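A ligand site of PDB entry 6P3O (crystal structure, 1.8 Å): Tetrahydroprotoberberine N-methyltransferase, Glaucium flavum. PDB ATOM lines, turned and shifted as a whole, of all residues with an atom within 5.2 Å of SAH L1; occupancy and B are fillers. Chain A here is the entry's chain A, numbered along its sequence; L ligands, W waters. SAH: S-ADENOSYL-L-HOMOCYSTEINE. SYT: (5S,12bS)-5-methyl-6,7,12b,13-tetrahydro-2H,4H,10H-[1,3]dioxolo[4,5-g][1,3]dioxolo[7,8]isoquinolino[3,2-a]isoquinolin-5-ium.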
ATOM      1  N   TYR A 106     -10.229 -27.425 -19.841  1.00  0.00           N
ATOM      2  CA  TYR A 106     -10.898 -27.722 -18.568  1.00  0.00           C
ATOM      3  C   TYR A 106     -11.592 -29.089 -18.612  1.00  0.00           C
ATOM      4  O   TYR A 106     -12.545 -29.352 -17.861  1.00  0.00           O
ATOM      5  CB  TYR A 106     -11.900 -26.605 -18.222  1.00  0.00           C
ATOM      6  CG  TYR A 106     -11.276 -25.312 -17.717  1.00  0.00           C
ATOM      7  CD1 TYR A 106     -10.844 -25.193 -16.388  1.00  0.00           C
ATOM      8  CD2 TYR A 106     -11.150 -24.202 -18.565  1.00  0.00           C
ATOM      9  CE1 TYR A 106     -10.283 -24.012 -15.924  1.00  0.00           C
ATOM     10  CE2 TYR A 106     -10.581 -23.014 -18.110  1.00  0.00           C
ATOM     11  CZ  TYR A 106     -10.151 -22.927 -16.788  1.00  0.00           C
ATOM     12  OH  TYR A 106      -9.599 -21.749 -16.324  1.00  0.00           O
ATOM     13  N   ILE A 121     -13.052 -29.404  -5.397  1.00  0.00           N
ATOM     14  CA  ILE A 121     -12.249 -29.132  -6.593  1.00  0.00           C
ATOM     15  C   ILE A 121     -12.390 -27.649  -7.027  1.00  0.00           C
ATOM     16  O   ILE A 121     -12.596 -27.329  -8.194  1.00  0.00           O
ATOM     17  CB  ILE A 121     -12.519 -30.126  -7.764  1.00  0.00           C
ATOM     18  CG1 ILE A 121     -12.809 -31.547  -7.260  1.00  0.00           C
ATOM     19  CG2 ILE A 121     -11.342 -30.138  -8.736  1.00  0.00           C
ATOM     20  CD1 ILE A 121     -13.321 -32.480  -8.338  1.00  0.00           C
ATOM     21  N   LYS A 122     -12.314 -26.763  -6.034  1.00  0.00           N
ATOM     22  CA  LYS A 122     -12.361 -25.337  -6.297  1.00  0.00           C
ATOM     23  C   LYS A 122     -11.092 -24.940  -7.054  1.00  0.00           C
ATOM     24  O   LYS A 122      -9.979 -25.322  -6.675  1.00  0.00           O
ATOM     25  CB  LYS A 122     -12.480 -24.572  -4.975  1.00  0.00           C
ATOM     26  CG  LYS A 122     -12.835 -23.108  -5.135  1.00  0.00           C
ATOM     27  CD  LYS A 122     -13.210 -22.542  -3.774  1.00  0.00           C
ATOM     28  CE  LYS A 122     -13.729 -21.120  -3.915  1.00  0.00           C
ATOM     29  NZ  LYS A 122     -12.621 -20.168  -4.255  1.00  0.00           N
ATOM     30  N   GLN A 123     -11.274 -24.206  -8.141  1.00  0.00           N
ATOM     31  CA  GLN A 123     -10.154 -23.769  -8.987  1.00  0.00           C
ATOM     32  C   GLN A 123     -10.145 -22.257  -9.035  1.00  0.00           C
ATOM     33  O   GLN A 123     -10.360 -21.624 -10.069  1.00  0.00           O
ATOM     34  CB  GLN A 123     -10.263 -24.387 -10.368  1.00  0.00           C
ATOM     35  CG  GLN A 123     -10.008 -25.883 -10.372  1.00  0.00           C
ATOM     36  CD  GLN A 123     -10.135 -26.478 -11.760  1.00  0.00           C
ATOM     37  OE1 GLN A 123     -11.236 -26.640 -12.266  1.00  0.00           O
ATOM     38  NE2 GLN A 123      -8.996 -26.798 -12.365  1.00  0.00           N
ATOM     39  N   SER A 124      -9.933 -21.693  -7.855  1.00  0.00           N
ATOM     40  CA  SER A 124      -9.949 -20.254  -7.638  1.00  0.00           C
ATOM     41  C   SER A 124      -9.382 -20.052  -6.251  1.00  0.00           C
ATOM     42  O   SER A 124      -9.302 -21.013  -5.462  1.00  0.00           O
ATOM     43  CB  SER A 124     -11.373 -19.691  -7.739  1.00  0.00           C
ATOM     44  OG  SER A 124     -12.281 -20.412  -6.930  1.00  0.00           O
ATOM     45  N   ASP A 160     -24.381 -19.118 -11.434  1.00  0.00           N
ATOM     46  CA  ASP A 160     -22.930 -19.094 -11.259  1.00  0.00           C
ATOM     47  C   ASP A 160     -22.282 -19.294 -12.614  1.00  0.00           C
ATOM     48  O   ASP A 160     -22.344 -20.380 -13.199  1.00  0.00           O
ATOM     49  CB  ASP A 160     -22.492 -20.165 -10.261  1.00  0.00           C
ATOM     50  CG  ASP A 160     -21.003 -20.109  -9.947  1.00  0.00           C
ATOM     51  OD1 ASP A 160     -20.290 -19.208 -10.429  1.00  0.00           O
ATOM     52  OD2 ASP A 160     -20.537 -20.968  -9.183  1.00  0.00           O
ATOM     53  N   ILE A 161     -21.656 -18.229 -13.103  1.00  0.00           N
ATOM     54  CA  ILE A 161     -21.090 -18.209 -14.457  1.00  0.00           C
ATOM     55  C   ILE A 161     -19.647 -18.700 -14.446  1.00  0.00           C
ATOM     56  O   ILE A 161     -18.789 -18.124 -13.776  1.00  0.00           O
ATOM     57  CB  ILE A 161     -21.224 -16.809 -15.103  1.00  0.00           C
ATOM     58  CG1 ILE A 161     -22.718 -16.539 -15.381  1.00  0.00           C
ATOM     59  CG2 ILE A 161     -20.391 -16.732 -16.380  1.00  0.00           C
ATOM     60  CD1 ILE A 161     -23.040 -15.158 -15.898  1.00  0.00           C
ATOM     61  N   GLY A 162     -19.412 -19.754 -15.232  1.00  0.00           N
ATOM     62  CA  GLY A 162     -18.121 -20.449 -15.228  1.00  0.00           C
ATOM     63  C   GLY A 162     -17.969 -21.159 -13.900  1.00  0.00           C
ATOM     64  O   GLY A 162     -17.023 -20.895 -13.156  1.00  0.00           O
ATOM     65  N   CYS A 163     -18.896 -22.057 -13.610  1.00  0.00           N
ATOM     66  CA  CYS A 163     -19.054 -22.661 -12.291  1.00  0.00           C
ATOM     67  C   CYS A 163     -18.009 -23.746 -11.951  1.00  0.00           C
ATOM     68  O   CYS A 163     -17.992 -24.250 -10.819  1.00  0.00           O
ATOM     69  CB  CYS A 163     -20.473 -23.218 -12.135  1.00  0.00           C
ATOM     70  SG  CYS A 163     -20.853 -24.463 -13.392  1.00  0.00           S
ATOM     71  N   GLY A 164     -17.168 -24.115 -12.913  1.00  0.00           N
ATOM     72  CA  GLY A 164     -16.105 -25.089 -12.688  1.00  0.00           C
ATOM     73  C   GLY A 164     -16.679 -26.431 -12.273  1.00  0.00           C
ATOM     74  O   GLY A 164     -17.649 -26.890 -12.867  1.00  0.00           O
ATOM     75  N   LEU A 184     -23.388 -22.423 -14.881  1.00  0.00           N
ATOM     76  CA  LEU A 184     -23.200 -22.356 -16.313  1.00  0.00           C
ATOM     77  C   LEU A 184     -21.723 -22.628 -16.603  1.00  0.00           C
ATOM     78  O   LEU A 184     -20.840 -21.970 -16.055  1.00  0.00           O
ATOM     79  CB  LEU A 184     -23.641 -21.003 -16.893  1.00  0.00           C
ATOM     80  CG  LEU A 184     -23.636 -20.848 -18.426  1.00  0.00           C
ATOM     81  CD1 LEU A 184     -24.667 -19.828 -18.888  1.00  0.00           C
ATOM     82  CD2 LEU A 184     -22.249 -20.479 -18.953  1.00  0.00           C
ATOM     83  N   THR A 185     -21.483 -23.596 -17.469  1.00  0.00           N
ATOM     84  CA  THR A 185     -20.127 -23.967 -17.863  1.00  0.00           C
ATOM     85  C   THR A 185     -20.103 -24.398 -19.315  1.00  0.00           C
ATOM     86  O   THR A 185     -21.111 -24.868 -19.850  1.00  0.00           O
ATOM     87  CB  THR A 185     -19.525 -25.078 -16.965  1.00  0.00           C
ATOM     88  OG1 THR A 185     -18.241 -25.463 -17.483  1.00  0.00           O
ATOM     89  CG2 THR A 185     -20.430 -26.306 -16.891  1.00  0.00           C
ATOM     90  N   ASN A 186     -18.946 -24.223 -19.956  1.00  0.00           N
ATOM     91  CA  ASN A 186     -18.752 -24.661 -21.327  1.00  0.00           C
ATOM     92  C   ASN A 186     -18.168 -26.076 -21.404  1.00  0.00           C
ATOM     93  O   ASN A 186     -17.887 -26.578 -22.500  1.00  0.00           O
ATOM     94  CB  ASN A 186     -17.893 -23.644 -22.109  1.00  0.00           C
ATOM     95  CG  ASN A 186     -16.501 -23.437 -21.516  1.00  0.00           C
ATOM     96  OD1 ASN A 186     -16.183 -23.908 -20.409  1.00  0.00           O
ATOM     97  ND2 ASN A 186     -15.650 -22.724 -22.258  1.00  0.00           N
ATOM     98  N   SER A 187     -17.993 -26.702 -20.242  1.00  0.00           N
ATOM     99  CA  SER A 187     -17.387 -28.027 -20.143  1.00  0.00           C
ATOM    100  C   SER A 187     -18.417 -29.114 -19.825  1.00  0.00           C
ATOM    101  O   SER A 187     -19.063 -29.067 -18.768  1.00  0.00           O
ATOM    102  CB  SER A 187     -16.278 -28.022 -19.088  1.00  0.00           C
ATOM    103  OG  SER A 187     -15.913 -29.347 -18.722  1.00  0.00           O
ATOM    104  N   GLN A 190     -17.455 -30.947 -16.618  1.00  0.00           N
ATOM    105  CA  GLN A 190     -17.849 -30.176 -15.440  1.00  0.00           C
ATOM    106  C   GLN A 190     -19.343 -30.295 -15.147  1.00  0.00           C
ATOM    107  O   GLN A 190     -19.718 -30.544 -14.006  1.00  0.00           O
ATOM    108  CB  GLN A 190     -17.435 -28.718 -15.583  1.00  0.00           C
ATOM    109  CG  GLN A 190     -15.937 -28.526 -15.427  1.00  0.00           C
ATOM    110  CD  GLN A 190     -15.496 -27.089 -15.564  1.00  0.00           C
ATOM    111  OE1 GLN A 190     -16.278 -26.209 -15.930  1.00  0.00           O
ATOM    112  NE2 GLN A 190     -14.229 -26.833 -15.258  1.00  0.00           N
ATOM    113  N   ALA A 211     -23.071 -24.223 -21.881  1.00  0.00           N
ATOM    114  CA  ALA A 211     -23.003 -23.141 -22.862  1.00  0.00           C
ATOM    115  C   ALA A 211     -21.688 -22.370 -22.785  1.00  0.00           C
ATOM    116  O   ALA A 211     -21.087 -22.249 -21.720  1.00  0.00           O
ATOM    117  CB  ALA A 211     -24.167 -22.172 -22.675  1.00  0.00           C
ATOM    118  N   ASP A 212     -21.260 -21.860 -23.938  1.00  0.00           N
ATOM    119  CA  ASP A 212     -20.304 -20.777 -23.989  1.00  0.00           C
ATOM    120  C   ASP A 212     -21.088 -19.541 -23.569  1.00  0.00           C
ATOM    121  O   ASP A 212     -22.046 -19.149 -24.250  1.00  0.00           O
ATOM    122  CB  ASP A 212     -19.754 -20.631 -25.419  1.00  0.00           C
ATOM    123  CG  ASP A 212     -18.687 -19.547 -25.560  1.00  0.00           C
ATOM    124  OD1 ASP A 212     -18.625 -18.591 -24.746  1.00  0.00           O
ATOM    125  OD2 ASP A 212     -17.910 -19.649 -26.532  1.00  0.00           O
ATOM    126  N   VAL A 213     -20.701 -18.940 -22.435  1.00  0.00           N
ATOM    127  CA  VAL A 213     -21.436 -17.790 -21.874  1.00  0.00           C
ATOM    128  C   VAL A 213     -21.549 -16.618 -22.864  1.00  0.00           C
ATOM    129  O   VAL A 213     -22.548 -15.887 -22.844  1.00  0.00           O
ATOM    130  CB  VAL A 213     -20.887 -17.336 -20.493  1.00  0.00           C
ATOM    131  CG1 VAL A 213     -19.553 -16.615 -20.599  1.00  0.00           C
ATOM    132  CG2 VAL A 213     -21.913 -16.469 -19.772  1.00  0.00           C
ATOM    133  N   THR A 214     -20.538 -16.464 -23.723  1.00  0.00           N
ATOM    134  CA  THR A 214     -20.507 -15.361 -24.697  1.00  0.00           C
ATOM    135  C   THR A 214     -21.511 -15.571 -25.843  1.00  0.00           C
ATOM    136  O   THR A 214     -21.852 -14.632 -26.550  1.00  0.00           O
ATOM    137  CB  THR A 214     -19.085 -15.126 -25.284  1.00  0.00           C
ATOM    138  OG1 THR A 214     -18.679 -16.271 -26.048  1.00  0.00           O
ATOM    139  CG2 THR A 214     -18.066 -14.862 -24.180  1.00  0.00           C
ATOM    140  N   ILE A 228     -16.950 -16.128 -10.578  1.00  0.00           N
ATOM    141  CA  ILE A 228     -15.765 -16.346  -9.734  1.00  0.00           C
ATOM    142  C   ILE A 228     -14.596 -16.767 -10.612  1.00  0.00           C
ATOM    143  O   ILE A 228     -14.532 -17.886 -11.111  1.00  0.00           O
ATOM    144  CB  ILE A 228     -15.981 -17.401  -8.604  1.00  0.00           C
ATOM    145  CG1 ILE A 228     -17.281 -17.150  -7.799  1.00  0.00           C
ATOM    146  CG2 ILE A 228     -14.766 -17.495  -7.695  1.00  0.00           C
ATOM    147  CD1 ILE A 228     -17.394 -15.827  -7.046  1.00  0.00           C
ATOM    148  N   GLU A 229     -13.679 -15.823 -10.805  1.00  0.00           N
ATOM    149  CA  GLU A 229     -12.466 -16.057 -11.596  1.00  0.00           C
ATOM    150  C   GLU A 229     -12.720 -16.643 -12.991  1.00  0.00           C
ATOM    151  O   GLU A 229     -12.017 -17.553 -13.467  1.00  0.00           O
ATOM    152  CB  GLU A 229     -11.421 -16.824 -10.759  1.00  0.00           C
ATOM    153  CG  GLU A 229     -10.912 -15.910  -9.633  1.00  0.00           C
ATOM    154  CD  GLU A 229     -10.100 -16.593  -8.541  1.00  0.00           C
ATOM    155  OE1 GLU A 229     -10.230 -16.182  -7.373  1.00  0.00           O
ATOM    156  OE2 GLU A 229      -9.309 -17.505  -8.860  1.00  0.00           O
ATOM    157  N   THR A 230     -13.751 -16.093 -13.628  1.00  0.00           N
ATOM    158  CA  THR A 230     -14.165 -16.433 -14.981  1.00  0.00           C
ATOM    159  C   THR A 230     -13.950 -15.240 -15.927  1.00  0.00           C
ATOM    160  O   THR A 230     -13.622 -15.426 -17.085  1.00  0.00           O
ATOM    161  CB  THR A 230     -15.635 -16.939 -15.007  1.00  0.00           C
ATOM    162  OG1 THR A 230     -15.699 -18.127 -14.203  1.00  0.00           O
ATOM    163  CG2 THR A 230     -16.111 -17.282 -16.420  1.00  0.00           C
ATOM    164  N   HIS A 233     -11.091 -14.779 -18.425  1.00  0.00           N
ATOM    165  CA  HIS A 233     -11.139 -15.495 -19.699  1.00  0.00           C
ATOM    166  C   HIS A 233     -11.970 -14.778 -20.756  1.00  0.00           C
ATOM    167  O   HIS A 233     -12.124 -15.280 -21.877  1.00  0.00           O
ATOM    168  CB  HIS A 233     -11.722 -16.899 -19.482  1.00  0.00           C
ATOM    169  CG  HIS A 233     -10.824 -17.816 -18.715  1.00  0.00           C
ATOM    170  ND1 HIS A 233      -9.621 -18.249 -19.209  1.00  0.00           N
ATOM    171  CD2 HIS A 233     -10.975 -18.382 -17.493  1.00  0.00           C
ATOM    172  CE1 HIS A 233      -9.051 -19.052 -18.316  1.00  0.00           C
ATOM    173  NE2 HIS A 233      -9.846 -19.142 -17.274  1.00  0.00           N
ATOM    174  N   MET A 234     -12.526 -13.623 -20.402  1.00  0.00           N
ATOM    175  CA  MET A 234     -13.455 -12.945 -21.300  1.00  0.00           C
ATOM    176  C   MET A 234     -12.736 -12.044 -22.284  1.00  0.00           C
ATOM    177  O   MET A 234     -12.029 -11.100 -21.901  1.00  0.00           O
ATOM    178  CB  MET A 234     -14.558 -12.209 -20.534  1.00  0.00           C
ATOM    179  CG  MET A 234     -15.479 -13.153 -19.780  1.00  0.00           C
ATOM    180  SD  MET A 234     -16.318 -14.332 -20.868  1.00  0.00           S
ATOM    181  CE  MET A 234     -15.807 -15.886 -20.147  1.00  0.00           C
HETATM  182  N   SAH L   1     -15.831 -20.550 -10.709  1.00  0.00           N
HETATM  183  CA  SAH L   1     -15.095 -21.856 -10.588  1.00  0.00           C
HETATM  184  CB  SAH L   1     -14.186 -22.088 -11.801  1.00  0.00           C
HETATM  185  CG  SAH L   1     -13.245 -20.941 -12.138  1.00  0.00           C
HETATM  186  SD  SAH L   1     -12.282 -21.461 -13.524  1.00  0.00           S
HETATM  187  C   SAH L   1     -14.287 -21.903  -9.320  1.00  0.00           C
HETATM  188  O   SAH L   1     -14.208 -20.906  -8.603  1.00  0.00           O
HETATM  189  OXT SAH L   1     -13.677 -22.913  -8.972  1.00  0.00           O
HETATM  190  C5' SAH L   1     -13.037 -20.598 -14.862  1.00  0.00           C
HETATM  191  C4' SAH L   1     -14.206 -21.423 -15.395  1.00  0.00           C
HETATM  192  O4' SAH L   1     -14.953 -20.695 -16.356  1.00  0.00           O
HETATM  193  C3' SAH L   1     -13.724 -22.718 -16.060  1.00  0.00           C
HETATM  194  O3' SAH L   1     -14.240 -23.819 -15.309  1.00  0.00           O
HETATM  195  C2' SAH L   1     -14.281 -22.697 -17.472  1.00  0.00           C
HETATM  196  O2' SAH L   1     -14.939 -23.924 -17.804  1.00  0.00           O
HETATM  197  C1' SAH L   1     -15.288 -21.556 -17.438  1.00  0.00           C
HETATM  198  N9  SAH L   1     -15.310 -20.784 -18.696  1.00  0.00           N
HETATM  199  C8  SAH L   1     -14.285 -20.163 -19.314  1.00  0.00           C
HETATM  200  N7  SAH L   1     -14.706 -19.546 -20.447  1.00  0.00           N
HETATM  201  C5  SAH L   1     -16.037 -19.775 -20.551  1.00  0.00           C
HETATM  202  C6  SAH L   1     -17.116 -19.423 -21.490  1.00  0.00           C
HETATM  203  N6  SAH L   1     -16.859 -18.666 -22.587  1.00  0.00           N
HETATM  204  N1  SAH L   1     -18.374 -19.876 -21.222  1.00  0.00           N
HETATM  205  C2  SAH L   1     -18.665 -20.622 -20.135  1.00  0.00           C
HETATM  206  N3  SAH L   1     -17.722 -20.976 -19.230  1.00  0.00           N
HETATM  207  C4  SAH L   1     -16.429 -20.598 -19.384  1.00  0.00           C
HETATM  208  C07 SYT L   2      -9.694 -19.972 -12.854  1.00  0.00           C
HETATM  209  N7  SYT L   2      -8.328 -19.578 -13.176  1.00  0.00           N
HETATM  210  C8  SYT L   2      -7.598 -20.719 -13.812  1.00  0.00           C
HETATM  211  C8A SYT L   2      -7.146 -21.763 -12.812  1.00  0.00           C
HETATM  212  C9  SYT L   2      -6.768 -23.032 -13.210  1.00  0.00           C
HETATM  213  O18 SYT L   2      -6.702 -23.594 -14.453  1.00  0.00           O
HETATM  214  C15 SYT L   2      -6.268 -25.010 -14.339  1.00  0.00           C
HETATM  215  O19 SYT L   2      -6.031 -25.183 -12.872  1.00  0.00           O
HETATM  216  C10 SYT L   2      -6.350 -24.028 -12.224  1.00  0.00           C
HETATM  217  C11 SYT L   2      -6.314 -23.746 -10.856  1.00  0.00           C
HETATM  218  C12 SYT L   2      -6.694 -22.470 -10.431  1.00  0.00           C
HETATM  219 C12A SYT L   2      -7.099 -21.472 -11.337  1.00  0.00           C
HETATM  220  C13 SYT L   2      -7.499 -20.112 -10.801  1.00  0.00           C
HETATM  221 C13A SYT L   2      -7.674 -19.071 -11.936  1.00  0.00           C
HETATM  222 C13B SYT L   2      -6.396 -18.357 -12.268  1.00  0.00           C
HETATM  223  C4A SYT L   2      -6.360 -17.531 -13.530  1.00  0.00           C
HETATM  224  C5  SYT L   2      -7.553 -17.440 -14.445  1.00  0.00           C
HETATM  225  C6  SYT L   2      -8.594 -18.533 -14.198  1.00  0.00           C
HETATM  226  C1  SYT L   2      -5.273 -18.428 -11.434  1.00  0.00           C
HETATM  227  C2  SYT L   2      -4.154 -17.713 -11.853  1.00  0.00           C
HETATM  228  O16 SYT L   2      -2.930 -17.608 -11.263  1.00  0.00           O
HETATM  229  C14 SYT L   2      -2.089 -16.795 -12.111  1.00  0.00           C
HETATM  230  O17 SYT L   2      -2.899 -16.348 -13.210  1.00  0.00           O
HETATM  231  C3  SYT L   2      -4.126 -16.925 -13.077  1.00  0.00           C
HETATM  232  C4  SYT L   2      -5.226 -16.828 -13.924  1.00  0.00           C
HETATM  233  O   HOH W   1     -17.866 -18.600 -11.223  1.00  0.00           O
HETATM  234  O   HOH W   2     -17.842 -20.622  -8.858  1.00  0.00           O
HETATM  235  O   HOH W   3     -16.171 -20.707  -6.490  1.00  0.00           O
HETATM  236  O   HOH W   4     -14.244 -25.508  -9.798  1.00  0.00           O
HETATM  237  O   HOH W   5     -16.893 -23.558 -15.586  1.00  0.00           O
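An oxygen (O) of SAH L1 is in hydrogen-bond range of the side-chain hydroxyl (OG) of Ser 124. The side-chain hydroxyl (OG1) of Thr 230 sits at hydrogen-bond distance from an oxygen (O4') of SAH L1. O2' of SAH L1 lies within hydrogen-bond range of OD1 of Asn 186. The side-chain amide nitrogen (NE2) of Gln 190 is in hydrogen-bond range of an oxygen (O3') of SAH L1 (3.0 Å). An oxygen (O19) of SYT L2 sits at hydrogen-bond distance from the side-chain amide nitrogen of Gln 123 (3.4 Å). A nitrogen (N) of SAH L1 is in hydrogen-bond range of the backbone carbonyl oxygen (O) of Gly 162 (2.7 Å). The backbone carbonyl oxygen (O) of Ile 228 is in hydrogen-bond range of a nitrogen (N) of SAH L1. The backbone NH of Val 213 is in hydrogen-bond range of a nitrogen (N1) of SAH L1, at 2.8 Å. The side-chain carboxylate of Asp 212 is in hydrogen-bond range of a nitrogen (N6) of SAH L1 (2.8 Å). The backbone NH (N) of Gln 123 lies within hydrogen-bond range of an oxygen (OXT) of SAH L1.
CD2 of Tyr 106 touches C2' of SAH L1, 3.6 Å away. C of Lys 122 touches OXT of SAH L1 (3.8 Å). Cys 163 touches SAH L1. CA of Gly 164 touches O3' of SAH L1, 3.5 Å away. Leu 184 touches SAH L1. Thr 185 touches SAH L1 (OG1 to O2', 3.7 Å). Ala 211 touches SAH L1. Glu 229 touches SAH L1. Met 234 touches SAH L1. Hydrophobic or aromatic side chains that line SAH L1: Tyr 106, Leu 184, Val 213, Ile 228 and Met 234.
Water W5 lies within hydrogen-bond range of an oxygen (O3') of SAH L1 (2.7 Å), the side-chain amide oxygen (OE1) of Gln 190 (2.7 Å), the backbone NH (N) of Gly 164 (2.7 Å), the side-chain hydroxyl (OG1) of Thr 185 (3.0 Å) and the backbone NH (N) of Cys 163 (3.2 Å). Water W2 lies within hydrogen-bond range of a nitrogen (N) of SAH L1 (2.7 Å) and the side-chain carboxylate (OD2) of Asp 160 (2.7 Å). Water W4 bridges OXT of SAH L1 (2.8 Å) and O of Ile 121 (2.9 Å).
N of Cys 163 lies within hydrogen-bond range of O of Leu 184, 3.1 Å away. The backbone carbonyl oxygen of Asp 160 sits at hydrogen-bond distance from the backbone NH of Leu 184 (2.8 Å). The backbone carbonyl oxygen (O) of Ala 211 sits close to the backbone NH (N) of Asn 186 (3.4 Å). A ring nitrogen (NE2) of His 233 sits at hydrogen-bond distance from the side-chain hydroxyl (OH) of Tyr 106 (2.8 Å). The side-chain hydroxyl (OG) of Ser 124 sits at hydrogen-bond distance from the side-chain amino group (NZ) of Lys 122, at 2.7 Å. The backbone carbonyl oxygen of Gly 162 lies within hydrogen-bond range of the side-chain hydroxyl of Thr 230, 3.2 Å away. N of Gln 190 is in hydrogen-bond range of OG of Ser 187 (3.1 Å). The side-chain amide oxygen (OE1) of Gln 190 lies close to the backbone carbonyl oxygen (O) of Gly 164.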
